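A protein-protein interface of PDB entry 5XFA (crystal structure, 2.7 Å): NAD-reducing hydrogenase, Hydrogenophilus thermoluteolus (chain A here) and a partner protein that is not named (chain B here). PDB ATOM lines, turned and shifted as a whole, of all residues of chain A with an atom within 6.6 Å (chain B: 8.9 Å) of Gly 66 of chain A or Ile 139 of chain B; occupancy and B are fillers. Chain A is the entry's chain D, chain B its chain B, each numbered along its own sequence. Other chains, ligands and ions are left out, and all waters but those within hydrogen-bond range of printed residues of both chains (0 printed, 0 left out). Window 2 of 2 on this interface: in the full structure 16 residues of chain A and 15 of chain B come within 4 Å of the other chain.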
ATOM      1  N   ALA A  62      11.662   6.645  17.998  1.00  0.00           N
ATOM      2  CA  ALA A  62      11.511   5.799  19.145  1.00  0.00           C
ATOM      3  C   ALA A  62      12.802   5.050  19.487  1.00  0.00           C
ATOM      4  O   ALA A  62      13.095   4.856  20.672  1.00  0.00           O
ATOM      5  CB  ALA A  62      10.386   4.822  18.905  1.00  0.00           C
ATOM      6  N   PHE A  63      13.566   4.653  18.466  1.00  0.00           N
ATOM      7  CA  PHE A  63      14.825   3.930  18.687  1.00  0.00           C
ATOM      8  C   PHE A  63      16.060   4.809  18.937  1.00  0.00           C
ATOM      9  O   PHE A  63      17.013   4.350  19.593  1.00  0.00           O
ATOM     10  CB  PHE A  63      15.071   2.833  17.620  1.00  0.00           C
ATOM     11  CG  PHE A  63      15.603   3.322  16.303  1.00  0.00           C
ATOM     12  CD1 PHE A  63      16.857   3.940  16.208  1.00  0.00           C
ATOM     13  CD2 PHE A  63      14.881   3.086  15.129  1.00  0.00           C
ATOM     14  CE1 PHE A  63      17.353   4.361  14.975  1.00  0.00           C
ATOM     15  CE2 PHE A  63      15.368   3.502  13.889  1.00  0.00           C
ATOM     16  CZ  PHE A  63      16.607   4.145  13.811  1.00  0.00           C
ATOM     17  N   ILE A  64      16.038   6.054  18.447  1.00  0.00           N
ATOM     18  CA  ILE A  64      17.030   7.088  18.837  1.00  0.00           C
ATOM     19  C   ILE A  64      16.991   7.432  20.340  1.00  0.00           C
ATOM     20  O   ILE A  64      17.931   7.999  20.879  1.00  0.00           O
ATOM     21  CB  ILE A  64      16.785   8.394  18.070  1.00  0.00           C
ATOM     22  CG1 ILE A  64      17.976   9.358  18.166  1.00  0.00           C
ATOM     23  CG2 ILE A  64      15.519   9.081  18.580  1.00  0.00           C
ATOM     24  CD1 ILE A  64      19.212   8.945  17.389  1.00  0.00           C
ATOM     25  N   VAL A  65      15.883   7.112  21.003  1.00  0.00           N
ATOM     26  CA  VAL A  65      15.778   7.345  22.415  1.00  0.00           C
ATOM     27  C   VAL A  65      16.672   6.344  23.100  1.00  0.00           C
ATOM     28  O   VAL A  65      16.667   5.164  22.748  1.00  0.00           O
ATOM     29  CB  VAL A  65      14.346   7.146  22.919  1.00  0.00           C
ATOM     30  CG1 VAL A  65      14.307   7.248  24.454  1.00  0.00           C
ATOM     31  CG2 VAL A  65      13.403   8.161  22.260  1.00  0.00           C
ATOM     32  N   GLY A  66      17.445   6.820  24.059  1.00  0.00           N
ATOM     33  CA  GLY A  66      18.354   5.965  24.776  1.00  0.00           C
ATOM     34  C   GLY A  66      19.782   6.251  24.368  1.00  0.00           C
ATOM     35  O   GLY A  66      20.720   5.923  25.134  1.00  0.00           O
ATOM     36  N   ARG A  67      19.956   6.854  23.191  1.00  0.00           N
ATOM     37  CA  ARG A  67      21.273   7.158  22.653  1.00  0.00           C
ATOM     38  C   ARG A  67      21.758   8.497  23.161  1.00  0.00           C
ATOM     39  O   ARG A  67      20.943   9.302  23.614  1.00  0.00           O
ATOM     40  CB  ARG A  67      21.222   7.266  21.119  1.00  0.00           C
ATOM     41  CG  ARG A  67      20.673   6.051  20.371  1.00  0.00           C
ATOM     42  CD  ARG A  67      21.406   4.770  20.736  1.00  0.00           C
ATOM     43  NE  ARG A  67      22.838   4.848  20.450  1.00  0.00           N
ATOM     44  CZ  ARG A  67      23.719   3.910  20.791  1.00  0.00           C
ATOM     45  NH1 ARG A  67      23.324   2.822  21.433  1.00  0.00           N
ATOM     46  NH2 ARG A  67      25.002   4.057  20.488  1.00  0.00           N
ATOM     47  N   PRO A  68      23.085   8.754  23.074  1.00  0.00           N
ATOM     48  CA  PRO A  68      23.593  10.058  23.475  1.00  0.00           C
ATOM     49  C   PRO A  68      23.195  11.116  22.505  1.00  0.00           C
ATOM     50  O   PRO A  68      23.068  10.837  21.304  1.00  0.00           O
ATOM     51  CB  PRO A  68      25.107   9.882  23.453  1.00  0.00           C
ATOM     52  CG  PRO A  68      25.351   8.707  22.575  1.00  0.00           C
ATOM     53  CD  PRO A  68      24.185   7.804  22.825  1.00  0.00           C
ATOM     54  N   LEU A 410      21.562  11.249  27.557  1.00  0.00           N
ATOM     55  CA  LEU A 410      20.844  10.373  26.646  1.00  0.00           C
ATOM     56  C   LEU A 410      19.498  10.994  26.295  1.00  0.00           C
ATOM     57  O   LEU A 410      18.728  11.400  27.163  1.00  0.00           O
ATOM     58  CB  LEU A 410      20.631   8.992  27.235  1.00  0.00           C
ATOM     59  CG  LEU A 410      21.898   8.269  27.711  1.00  0.00           C
ATOM     60  CD1 LEU A 410      21.580   6.883  28.246  1.00  0.00           C
ATOM     61  CD2 LEU A 410      22.948   8.182  26.618  1.00  0.00           C
ATOM     62  N   ILE A 411      19.224  11.042  25.000  1.00  0.00           N
ATOM     63  CA  ILE A 411      17.979  11.518  24.485  1.00  0.00           C
ATOM     64  C   ILE A 411      16.853  10.780  25.168  1.00  0.00           C
ATOM     65  O   ILE A 411      16.881   9.552  25.252  1.00  0.00           O
ATOM     66  CB  ILE A 411      17.892  11.202  22.994  1.00  0.00           C
ATOM     67  CG1 ILE A 411      18.907  12.039  22.228  1.00  0.00           C
ATOM     68  CG2 ILE A 411      16.498  11.467  22.467  1.00  0.00           C
ATOM     69  CD1 ILE A 411      19.267  11.440  20.895  1.00  0.00           C
ATOM     70  N   THR A 412      15.855  11.524  25.638  1.00  0.00           N
ATOM     71  CA  THR A 412      14.685  10.935  26.302  1.00  0.00           C
ATOM     72  C   THR A 412      13.475  11.009  25.429  1.00  0.00           C
ATOM     73  O   THR A 412      12.482  10.344  25.703  1.00  0.00           O
ATOM     74  CB  THR A 412      14.317  11.699  27.571  1.00  0.00           C
ATOM     75  OG1 THR A 412      13.975  13.035  27.202  1.00  0.00           O
ATOM     76  CG2 THR A 412      15.469  11.705  28.562  1.00  0.00           C
ATOM     77  N   TYR A 413      13.538  11.848  24.398  1.00  0.00           N
ATOM     78  CA  TYR A 413      12.411  12.044  23.478  1.00  0.00           C
ATOM     79  C   TYR A 413      12.845  12.682  22.159  1.00  0.00           C
ATOM     80  O   TYR A 413      13.562  13.673  22.133  1.00  0.00           O
ATOM     81  CB  TYR A 413      11.352  12.935  24.132  1.00  0.00           C
ATOM     82  CG  TYR A 413      10.164  13.227  23.225  1.00  0.00           C
ATOM     83  CD1 TYR A 413       9.166  12.282  23.041  1.00  0.00           C
ATOM     84  CD2 TYR A 413      10.041  14.444  22.571  1.00  0.00           C
ATOM     85  CE1 TYR A 413       8.087  12.542  22.239  1.00  0.00           C
ATOM     86  CE2 TYR A 413       8.960  14.710  21.754  1.00  0.00           C
ATOM     87  CZ  TYR A 413       7.998  13.747  21.604  1.00  0.00           C
ATOM     88  OH  TYR A 413       6.938  13.977  20.813  1.00  0.00           O
ATOM     89  N   GLN B 136      21.455  -7.191  23.641  1.00  0.00           N
ATOM     90  CA  GLN B 136      20.497  -6.221  24.132  1.00  0.00           C
ATOM     91  C   GLN B 136      20.917  -5.677  25.494  1.00  0.00           C
ATOM     92  O   GLN B 136      20.132  -5.625  26.436  1.00  0.00           O
ATOM     93  CB  GLN B 136      19.095  -6.856  24.145  1.00  0.00           C
ATOM     94  CG  GLN B 136      18.534  -7.093  22.742  1.00  0.00           C
ATOM     95  CD  GLN B 136      17.105  -7.597  22.740  1.00  0.00           C
ATOM     96  OE1 GLN B 136      16.567  -7.966  23.781  1.00  0.00           O
ATOM     97  NE2 GLN B 136      16.486  -7.626  21.559  1.00  0.00           N
ATOM     98  N   ARG B 137      22.166  -5.248  25.578  1.00  0.00           N
ATOM     99  CA  ARG B 137      22.717  -4.751  26.833  1.00  0.00           C
ATOM    100  C   ARG B 137      22.448  -3.277  26.950  1.00  0.00           C
ATOM    101  O   ARG B 137      22.319  -2.576  25.950  1.00  0.00           O
ATOM    102  CB  ARG B 137      24.219  -4.967  26.887  1.00  0.00           C
ATOM    103  CG  ARG B 137      24.632  -6.417  26.942  1.00  0.00           C
ATOM    104  CD  ARG B 137      25.582  -6.741  25.801  1.00  0.00           C
ATOM    105  NE  ARG B 137      26.707  -7.540  26.243  1.00  0.00           N
ATOM    106  CZ  ARG B 137      27.631  -8.030  25.431  1.00  0.00           C
ATOM    107  NH1 ARG B 137      27.555  -7.823  24.122  1.00  0.00           N
ATOM    108  NH2 ARG B 137      28.640  -8.737  25.942  1.00  0.00           N
ATOM    109  N   ARG B 138      22.394  -2.810  28.189  1.00  0.00           N
ATOM    110  CA  ARG B 138      22.008  -1.442  28.465  1.00  0.00           C
ATOM    111  C   ARG B 138      23.217  -0.533  28.494  1.00  0.00           C
ATOM    112  O   ARG B 138      24.261  -0.878  29.048  1.00  0.00           O
ATOM    113  CB  ARG B 138      21.249  -1.371  29.794  1.00  0.00           C
ATOM    114  CG  ARG B 138      19.766  -1.670  29.668  1.00  0.00           C
ATOM    115  CD  ARG B 138      19.001  -0.395  29.348  1.00  0.00           C
ATOM    116  NE  ARG B 138      17.757  -0.325  30.103  1.00  0.00           N
ATOM    117  CZ  ARG B 138      17.619   0.226  31.313  1.00  0.00           C
ATOM    118  NH1 ARG B 138      18.646   0.791  31.956  1.00  0.00           N
ATOM    119  NH2 ARG B 138      16.422   0.210  31.891  1.00  0.00           N
ATOM    120  N   ILE B 139      23.067   0.633  27.891  1.00  0.00           N
ATOM    121  CA  ILE B 139      24.039   1.714  28.031  1.00  0.00           C
ATOM    122  C   ILE B 139      24.134   2.147  29.489  1.00  0.00           C
ATOM    123  O   ILE B 139      23.138   2.085  30.225  1.00  0.00           O
ATOM    124  CB  ILE B 139      23.618   2.908  27.163  1.00  0.00           C
ATOM    125  CG1 ILE B 139      23.806   2.543  25.702  1.00  0.00           C
ATOM    126  CG2 ILE B 139      24.438   4.141  27.479  1.00  0.00           C
ATOM    127  CD1 ILE B 139      23.089   3.465  24.767  1.00  0.00           C
ATOM    128  N   ASP B 140      25.317   2.579  29.910  1.00  0.00           N
ATOM    129  CA  ASP B 140      25.483   3.096  31.246  1.00  0.00           C
ATOM    130  C   ASP B 140      26.010   4.503  31.159  1.00  0.00           C
ATOM    131  O   ASP B 140      27.218   4.728  30.959  1.00  0.00           O
ATOM    132  CB  ASP B 140      26.417   2.232  32.068  1.00  0.00           C
ATOM    133  CG  ASP B 140      26.592   2.761  33.470  1.00  0.00           C
ATOM    134  OD1 ASP B 140      26.370   3.967  33.702  1.00  0.00           O
ATOM    135  OD2 ASP B 140      26.941   1.970  34.365  1.00  0.00           O
ATOM    136  N   ALA B 141      25.098   5.464  31.329  1.00  0.00           N
ATOM    137  CA  ALA B 141      25.471   6.862  31.261  1.00  0.00           C
ATOM    138  C   ALA B 141      25.385   7.504  32.621  1.00  0.00           C
ATOM    139  O   ALA B 141      25.057   8.674  32.725  1.00  0.00           O
ATOM    140  CB  ALA B 141      24.603   7.584  30.258  1.00  0.00           C
ATOM    141  N   SER B 142      25.749   6.745  33.660  1.00  0.00           N
ATOM    142  CA  SER B 142      25.613   7.196  35.049  1.00  0.00           C
ATOM    143  C   SER B 142      26.779   8.028  35.514  1.00  0.00           C
ATOM    144  O   SER B 142      26.634   8.867  36.385  1.00  0.00           O
ATOM    145  CB  SER B 142      25.489   6.013  35.969  1.00  0.00           C
ATOM    146  OG  SER B 142      26.718   5.327  35.999  1.00  0.00           O
ATOM    147  N   HIS B 143      27.950   7.781  34.952  1.00  0.00           N
ATOM    148  CA  HIS B 143      29.125   8.591  35.269  1.00  0.00           C
ATOM    149  C   HIS B 143      28.972   9.997  34.664  1.00  0.00           C
ATOM    150  O   HIS B 143      28.447  10.138  33.554  1.00  0.00           O
ATOM    151  CB  HIS B 143      30.373   7.906  34.734  1.00  0.00           C
ATOM    152  CG  HIS B 143      31.636   8.462  35.275  1.00  0.00           C
ATOM    153  ND1 HIS B 143      32.332   9.461  34.642  1.00  0.00           N
ATOM    154  CD2 HIS B 143      32.325   8.179  36.404  1.00  0.00           C
ATOM    155  CE1 HIS B 143      33.399   9.772  35.353  1.00  0.00           C
ATOM    156  NE2 HIS B 143      33.422   9.001  36.425  1.00  0.00           N
ATOM    157  N   LEU B 146      31.535  10.126  31.459  1.00  0.00           N
ATOM    158  CA  LEU B 146      31.870   8.912  30.740  1.00  0.00           C
ATOM    159  C   LEU B 146      30.663   8.091  30.478  1.00  0.00           C
ATOM    160  O   LEU B 146      29.737   8.064  31.301  1.00  0.00           O
ATOM    161  CB  LEU B 146      32.817   8.025  31.592  1.00  0.00           C
ATOM    162  CG  LEU B 146      34.246   8.484  31.853  1.00  0.00           C
ATOM    163  CD1 LEU B 146      34.917   7.522  32.806  1.00  0.00           C
ATOM    164  CD2 LEU B 146      35.001   8.556  30.528  1.00  0.00           C
ATOM    165  N   TRP B 147      30.702   7.350  29.378  1.00  0.00           N
ATOM    166  CA  TRP B 147      29.608   6.484  29.080  1.00  0.00           C
ATOM    167  C   TRP B 147      30.094   5.250  28.423  1.00  0.00           C
ATOM    168  O   TRP B 147      31.130   5.274  27.777  1.00  0.00           O
ATOM    169  CB  TRP B 147      28.549   7.227  28.211  1.00  0.00           C
ATOM    170  CG  TRP B 147      28.854   7.362  26.800  1.00  0.00           C
ATOM    171  CD1 TRP B 147      29.709   8.229  26.243  1.00  0.00           C
ATOM    172  CD2 TRP B 147      28.269   6.612  25.740  1.00  0.00           C
ATOM    173  NE1 TRP B 147      29.716   8.062  24.886  1.00  0.00           N
ATOM    174  CE2 TRP B 147      28.834   7.073  24.549  1.00  0.00           C
ATOM    175  CE3 TRP B 147      27.294   5.609  25.680  1.00  0.00           C
ATOM    176  CZ2 TRP B 147      28.471   6.561  23.282  1.00  0.00           C
ATOM    177  CZ3 TRP B 147      26.942   5.072  24.430  1.00  0.00           C
ATOM    178  CH2 TRP B 147      27.529   5.560  23.246  1.00  0.00           C
ATOM    179  N   LEU B 148      29.284   4.196  28.545  1.00  0.00           N
ATOM    180  CA  LEU B 148      29.645   2.845  28.143  1.00  0.00           C
ATOM    181  C   LEU B 148      28.580   2.171  27.335  1.00  0.00           C
ATOM    182  O   LEU B 148      27.544   1.830  27.875  1.00  0.00           O
ATOM    183  CB  LEU B 148      29.872   1.982  29.400  1.00  0.00           C
ATOM    184  CG  LEU B 148      30.102   0.470  29.195  1.00  0.00           C
ATOM    185  CD1 LEU B 148      31.447   0.174  28.541  1.00  0.00           C
ATOM    186  CD2 LEU B 148      29.999  -0.246  30.537  1.00  0.00           C
ATOM    187  N   ASP B 149      28.830   1.979  26.043  1.00  0.00           N
ATOM    188  CA  ASP B 149      27.951   1.145  25.192  1.00  0.00           C
ATOM    189  C   ASP B 149      28.525  -0.258  25.234  1.00  0.00           C
ATOM    190  O   ASP B 149      29.593  -0.495  24.691  1.00  0.00           O
ATOM    191  CB  ASP B 149      27.879   1.641  23.725  1.00  0.00           C
ATOM    192  CG  ASP B 149      26.812   0.907  22.910  1.00  0.00           C
ATOM    193  OD1 ASP B 149      26.416  -0.218  23.286  1.00  0.00           O
ATOM    194  OD2 ASP B 149      26.346   1.460  21.889  1.00  0.00           O
ATOM    195  N   PRO B 150      27.825  -1.201  25.853  1.00  0.00           N
ATOM    196  CA  PRO B 150      28.437  -2.505  26.003  1.00  0.00           C
ATOM    197  C   PRO B 150      28.221  -3.425  24.840  1.00  0.00           C
ATOM    198  O   PRO B 150      28.810  -4.528  24.821  1.00  0.00           O
ATOM    199  CB  PRO B 150      27.755  -3.075  27.237  1.00  0.00           C
ATOM    200  CG  PRO B 150      26.752  -2.061  27.667  1.00  0.00           C
ATOM    201  CD  PRO B 150      26.525  -1.151  26.518  1.00  0.00           C
ATOM    202  N   ASN B 151      27.442  -2.977  23.856  1.00  0.00           N
ATOM    203  CA  ASN B 151      27.166  -3.777  22.658  1.00  0.00           C
ATOM    204  C   ASN B 151      28.246  -3.651  21.590  1.00  0.00           C
ATOM    205  O   ASN B 151      28.212  -4.353  20.578  1.00  0.00           O
ATOM    206  CB  ASN B 151      25.795  -3.412  22.086  1.00  0.00           C
ATOM    207  CG  ASN B 151      24.661  -3.825  23.006  1.00  0.00           C
ATOM    208  OD1 ASN B 151      24.504  -5.019  23.317  1.00  0.00           O
ATOM    209  ND2 ASN B 151      23.917  -2.856  23.502  1.00  0.00           N
ATOM    210  N   ARG B 152      29.192  -2.752  21.848  1.00  0.00           N
ATOM    211  CA  ARG B 152      30.406  -2.579  21.072  1.00  0.00           C
ATOM    212  C   ARG B 152      31.654  -3.229  21.726  1.00  0.00           C
ATOM    213  O   ARG B 152      32.688  -3.377  21.078  1.00  0.00           O
ATOM    214  CB  ARG B 152      30.651  -1.074  20.897  1.00  0.00           C
ATOM    215  CG  ARG B 152      29.625  -0.403  19.987  1.00  0.00           C
ATOM    216  CD  ARG B 152      29.727   1.097  20.057  1.00  0.00           C
ATOM    217  NE  ARG B 152      28.756   1.759  19.186  1.00  0.00           N
ATOM    218  CZ  ARG B 152      28.494   3.064  19.241  1.00  0.00           C
ATOM    219  NH1 ARG B 152      29.136   3.847  20.110  1.00  0.00           N
ATOM    220  NH2 ARG B 152      27.607   3.605  18.421  1.00  0.00           N
ATOM    221  N   ARG B 181      30.117 -10.013  29.846  1.00  0.00           N
ATOM    222  CA  ARG B 181      30.039  -8.572  29.594  1.00  0.00           C
ATOM    223  C   ARG B 181      30.865  -7.780  30.575  1.00  0.00           C
ATOM    224  O   ARG B 181      31.170  -8.273  31.666  1.00  0.00           O
ATOM    225  CB  ARG B 181      28.594  -8.115  29.693  1.00  0.00           C
ATOM    226  CG  ARG B 181      27.956  -8.239  31.073  1.00  0.00           C
ATOM    227  CD  ARG B 181      26.738  -7.327  31.160  1.00  0.00           C
ATOM    228  NE  ARG B 181      27.128  -5.911  31.041  1.00  0.00           N
ATOM    229  CZ  ARG B 181      26.305  -4.897  30.759  1.00  0.00           C
ATOM    230  NH1 ARG B 181      25.002  -5.110  30.552  1.00  0.00           N
ATOM    231  NH2 ARG B 181      26.791  -3.655  30.685  1.00  0.00           N
ATOM    232  N   GLY B 189      26.158  -1.537  40.493  1.00  0.00           N
ATOM    233  CA  GLY B 189      26.425  -1.902  39.104  1.00  0.00           C
ATOM    234  C   GLY B 189      26.518  -0.708  38.165  1.00  0.00           C
ATOM    235  O   GLY B 189      26.440  -0.857  36.956  1.00  0.00           O
ATOM    236  N   ARG B 190      26.734   0.481  38.715  1.00  0.00           N
ATOM    237  CA  ARG B 190      26.729   1.692  37.924  1.00  0.00           C
ATOM    238  C   ARG B 190      28.114   2.306  37.962  1.00  0.00           C
ATOM    239  O   ARG B 190      28.634   2.561  39.020  1.00  0.00           O
ATOM    240  CB  ARG B 190      25.709   2.671  38.501  1.00  0.00           C
ATOM    241  CG  ARG B 190      24.306   2.111  38.634  1.00  0.00           C
ATOM    242  CD  ARG B 190      23.363   2.835  37.699  1.00  0.00           C
ATOM    243  NE  ARG B 190      23.579   2.422  36.311  1.00  0.00           N
ATOM    244  CZ  ARG B 190      23.050   3.010  35.238  1.00  0.00           C
ATOM    245  NH1 ARG B 190      22.270   4.080  35.348  1.00  0.00           N
ATOM    246  NH2 ARG B 190      23.316   2.524  34.032  1.00  0.00           N
ATOM    247  N   LEU B 191      28.698   2.569  36.807  1.00  0.00           N
ATOM    248  CA  LEU B 191      29.995   3.244  36.737  1.00  0.00           C
ATOM    249  C   LEU B 191      30.122   4.463  37.625  1.00  0.00           C
ATOM    250  O   LEU B 191      31.180   4.691  38.165  1.00  0.00           O
ATOM    251  CB  LEU B 191      30.272   3.714  35.314  1.00  0.00           C
ATOM    252  CG  LEU B 191      30.619   2.635  34.292  1.00  0.00           C
ATOM    253  CD1 LEU B 191      30.627   3.226  32.889  1.00  0.00           C
ATOM    254  CD2 LEU B 191      31.963   2.007  34.640  1.00  0.00           C
ATOM    255  N   GLY B 209      34.660   1.587  20.399  1.00  0.00           N
ATOM    256  CA  GLY B 209      33.675   2.588  20.846  1.00  0.00           C
ATOM    257  C   GLY B 209      32.836   2.213  22.080  1.00  0.00           C
ATOM    258  O   GLY B 209      31.783   2.784  22.305  1.00  0.00           O
ATOM    259  N   ALA B 210      33.337   1.298  22.902  1.00  0.00           N
ATOM    260  CA  ALA B 210      32.622   0.850  24.095  1.00  0.00           C
ATOM    261  C   ALA B 210      32.652   1.888  25.189  1.00  0.00           C
ATOM    262  O   ALA B 210      31.615   2.478  25.501  1.00  0.00           O
ATOM    263  CB  ALA B 210      33.212  -0.440  24.622  1.00  0.00           C
ATOM    264  N   ASN B 212      33.639   5.483  26.482  1.00  0.00           N
ATOM    265  CA  ASN B 212      33.966   6.780  25.952  1.00  0.00           C
ATOM    266  C   ASN B 212      33.776   7.934  26.931  1.00  0.00           C
ATOM    267  O   ASN B 212      32.959   7.836  27.845  1.00  0.00           O
ATOM    268  CB  ASN B 212      33.118   7.038  24.687  1.00  0.00           C
ATOM    269  CG  ASN B 212      32.969   5.809  23.840  1.00  0.00           C
ATOM    270  OD1 ASN B 212      33.893   5.430  23.136  1.00  0.00           O
ATOM    271  ND2 ASN B 212      31.819   5.152  23.933  1.00  0.00           N
ATOM    272  N   LYS B 214      32.155  11.645  27.525  1.00  0.00           N
ATOM    273  CA  LYS B 214      30.890  12.207  27.158  1.00  0.00           C
ATOM    274  C   LYS B 214      31.129  13.507  26.423  1.00  0.00           C
ATOM    275  O   LYS B 214      31.999  14.287  26.823  1.00  0.00           O
ATOM    276  CB  LYS B 214      30.025  12.453  28.386  1.00  0.00           C
ATOM    277  CG  LYS B 214      29.210  11.246  28.825  1.00  0.00           C
ATOM    278  CD  LYS B 214      28.211  11.624  29.907  1.00  0.00           C
ATOM    279  CE  LYS B 214      27.397  10.416  30.349  1.00  0.00           C
ATOM    280  NZ  LYS B 214      26.840  10.626  31.717  1.00  0.00           N
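The side-chain amino group (NZ) of Lys 214 of chain B lies within hydrogen-bond range of the backbone carbonyl oxygen (O) of Ala 141 of chain B (2.8 Å).
The side-chain carboxylate (OD1) of Asp 149 of chain B is in hydrogen-bond range of the backbone NH (N) of Asn 151 of chain B (3.0 Å).
The side-chain carboxylate (OD2) of Asp 149 of chain B is in salt-bridge range of the guanidinium group (NE) of Arg 152 of chain B.
The backbone NH (N) of Asp 149 of chain B is in hydrogen-bond range of the backbone carbonyl oxygen (O) of Ala 210 of chain B.
The backbone NH (N) of Gly 66 of chain A sits at hydrogen-bond distance from the backbone carbonyl oxygen (O) of Ile 411 of chain A, 3.0 Å away.
The backbone carbonyl oxygen of Arg 67 of chain A sits at hydrogen-bond distance from the backbone NH of Ile 411 of chain A (2.8 Å).
OD2 of Asp 149 of chain B lies within salt-bridge range of NH2 of Arg 67 of chain A, at 3.2 Å.
The guanidinium group (NH2) of Arg 67 of chain A lies close to the guanidinium group (NH2) of Arg 152 of chain B (3.4 Å).
No residue of chain B comes within 4 Å of Val 65 of chain A.
Gly 66 of chain A touches just one residue of chain B: Ile 139.
Arg 67 of chain A touches just these residues of chain B: Ile 139 (3.4 Å), Asp 149 (3.2 Å) and Arg 152 (3.4 Å).
Of the printed residues of chain B, Pro 68 of chain A touches Trp 147 (3.9 Å).
Printed residues of chain B within 4 Å of Leu 410 of chain A: Ala 141.
Tyr 413 of chain A touches none of the printed residues of chain B.
Printed residues of chain A within 4 Å of Ile 139 of chain B: Gly 66 (3.4 Å) and Arg 67 (3.4 Å).
Of the printed residues of chain A, Ala 141 of chain B touches Leu 410 (3.7 Å).
Ser 142 of chain B touches none of the printed residues of chain A.
Of the printed residues of chain A, Asp 149 of chain B touches Arg 67 (3.2 Å).
Of the printed residues of chain A, Arg 152 of chain B touches Arg 67 (3.4 Å).
Among the printed residues, pairs that only touch across the chains: Arg 67 of chain A with Ile 139 of chain B (3.4 Å), Gly 66 of chain A with Ile 139 of chain B (3.4 Å), Leu 410 of chain A with Ala 141 of chain B (3.7 Å) and Pro 68 of chain A with Trp 147 of chain B (3.9 Å).
Printed residues of chain B that touch a printed residue of chain A: Ile 139, Ala 141, Trp 147, Asp 149 and Arg 152.
Of the 11 printed residues of chain A, 4 touch a printed residue of chain B.
Among the printed residues, Asp or Glu carboxylates within 4 Å of a Lys or Arg side-chain nitrogen of the other chain: Arg 67 of chain A with Asp 149 of chain B (3.2 Å).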
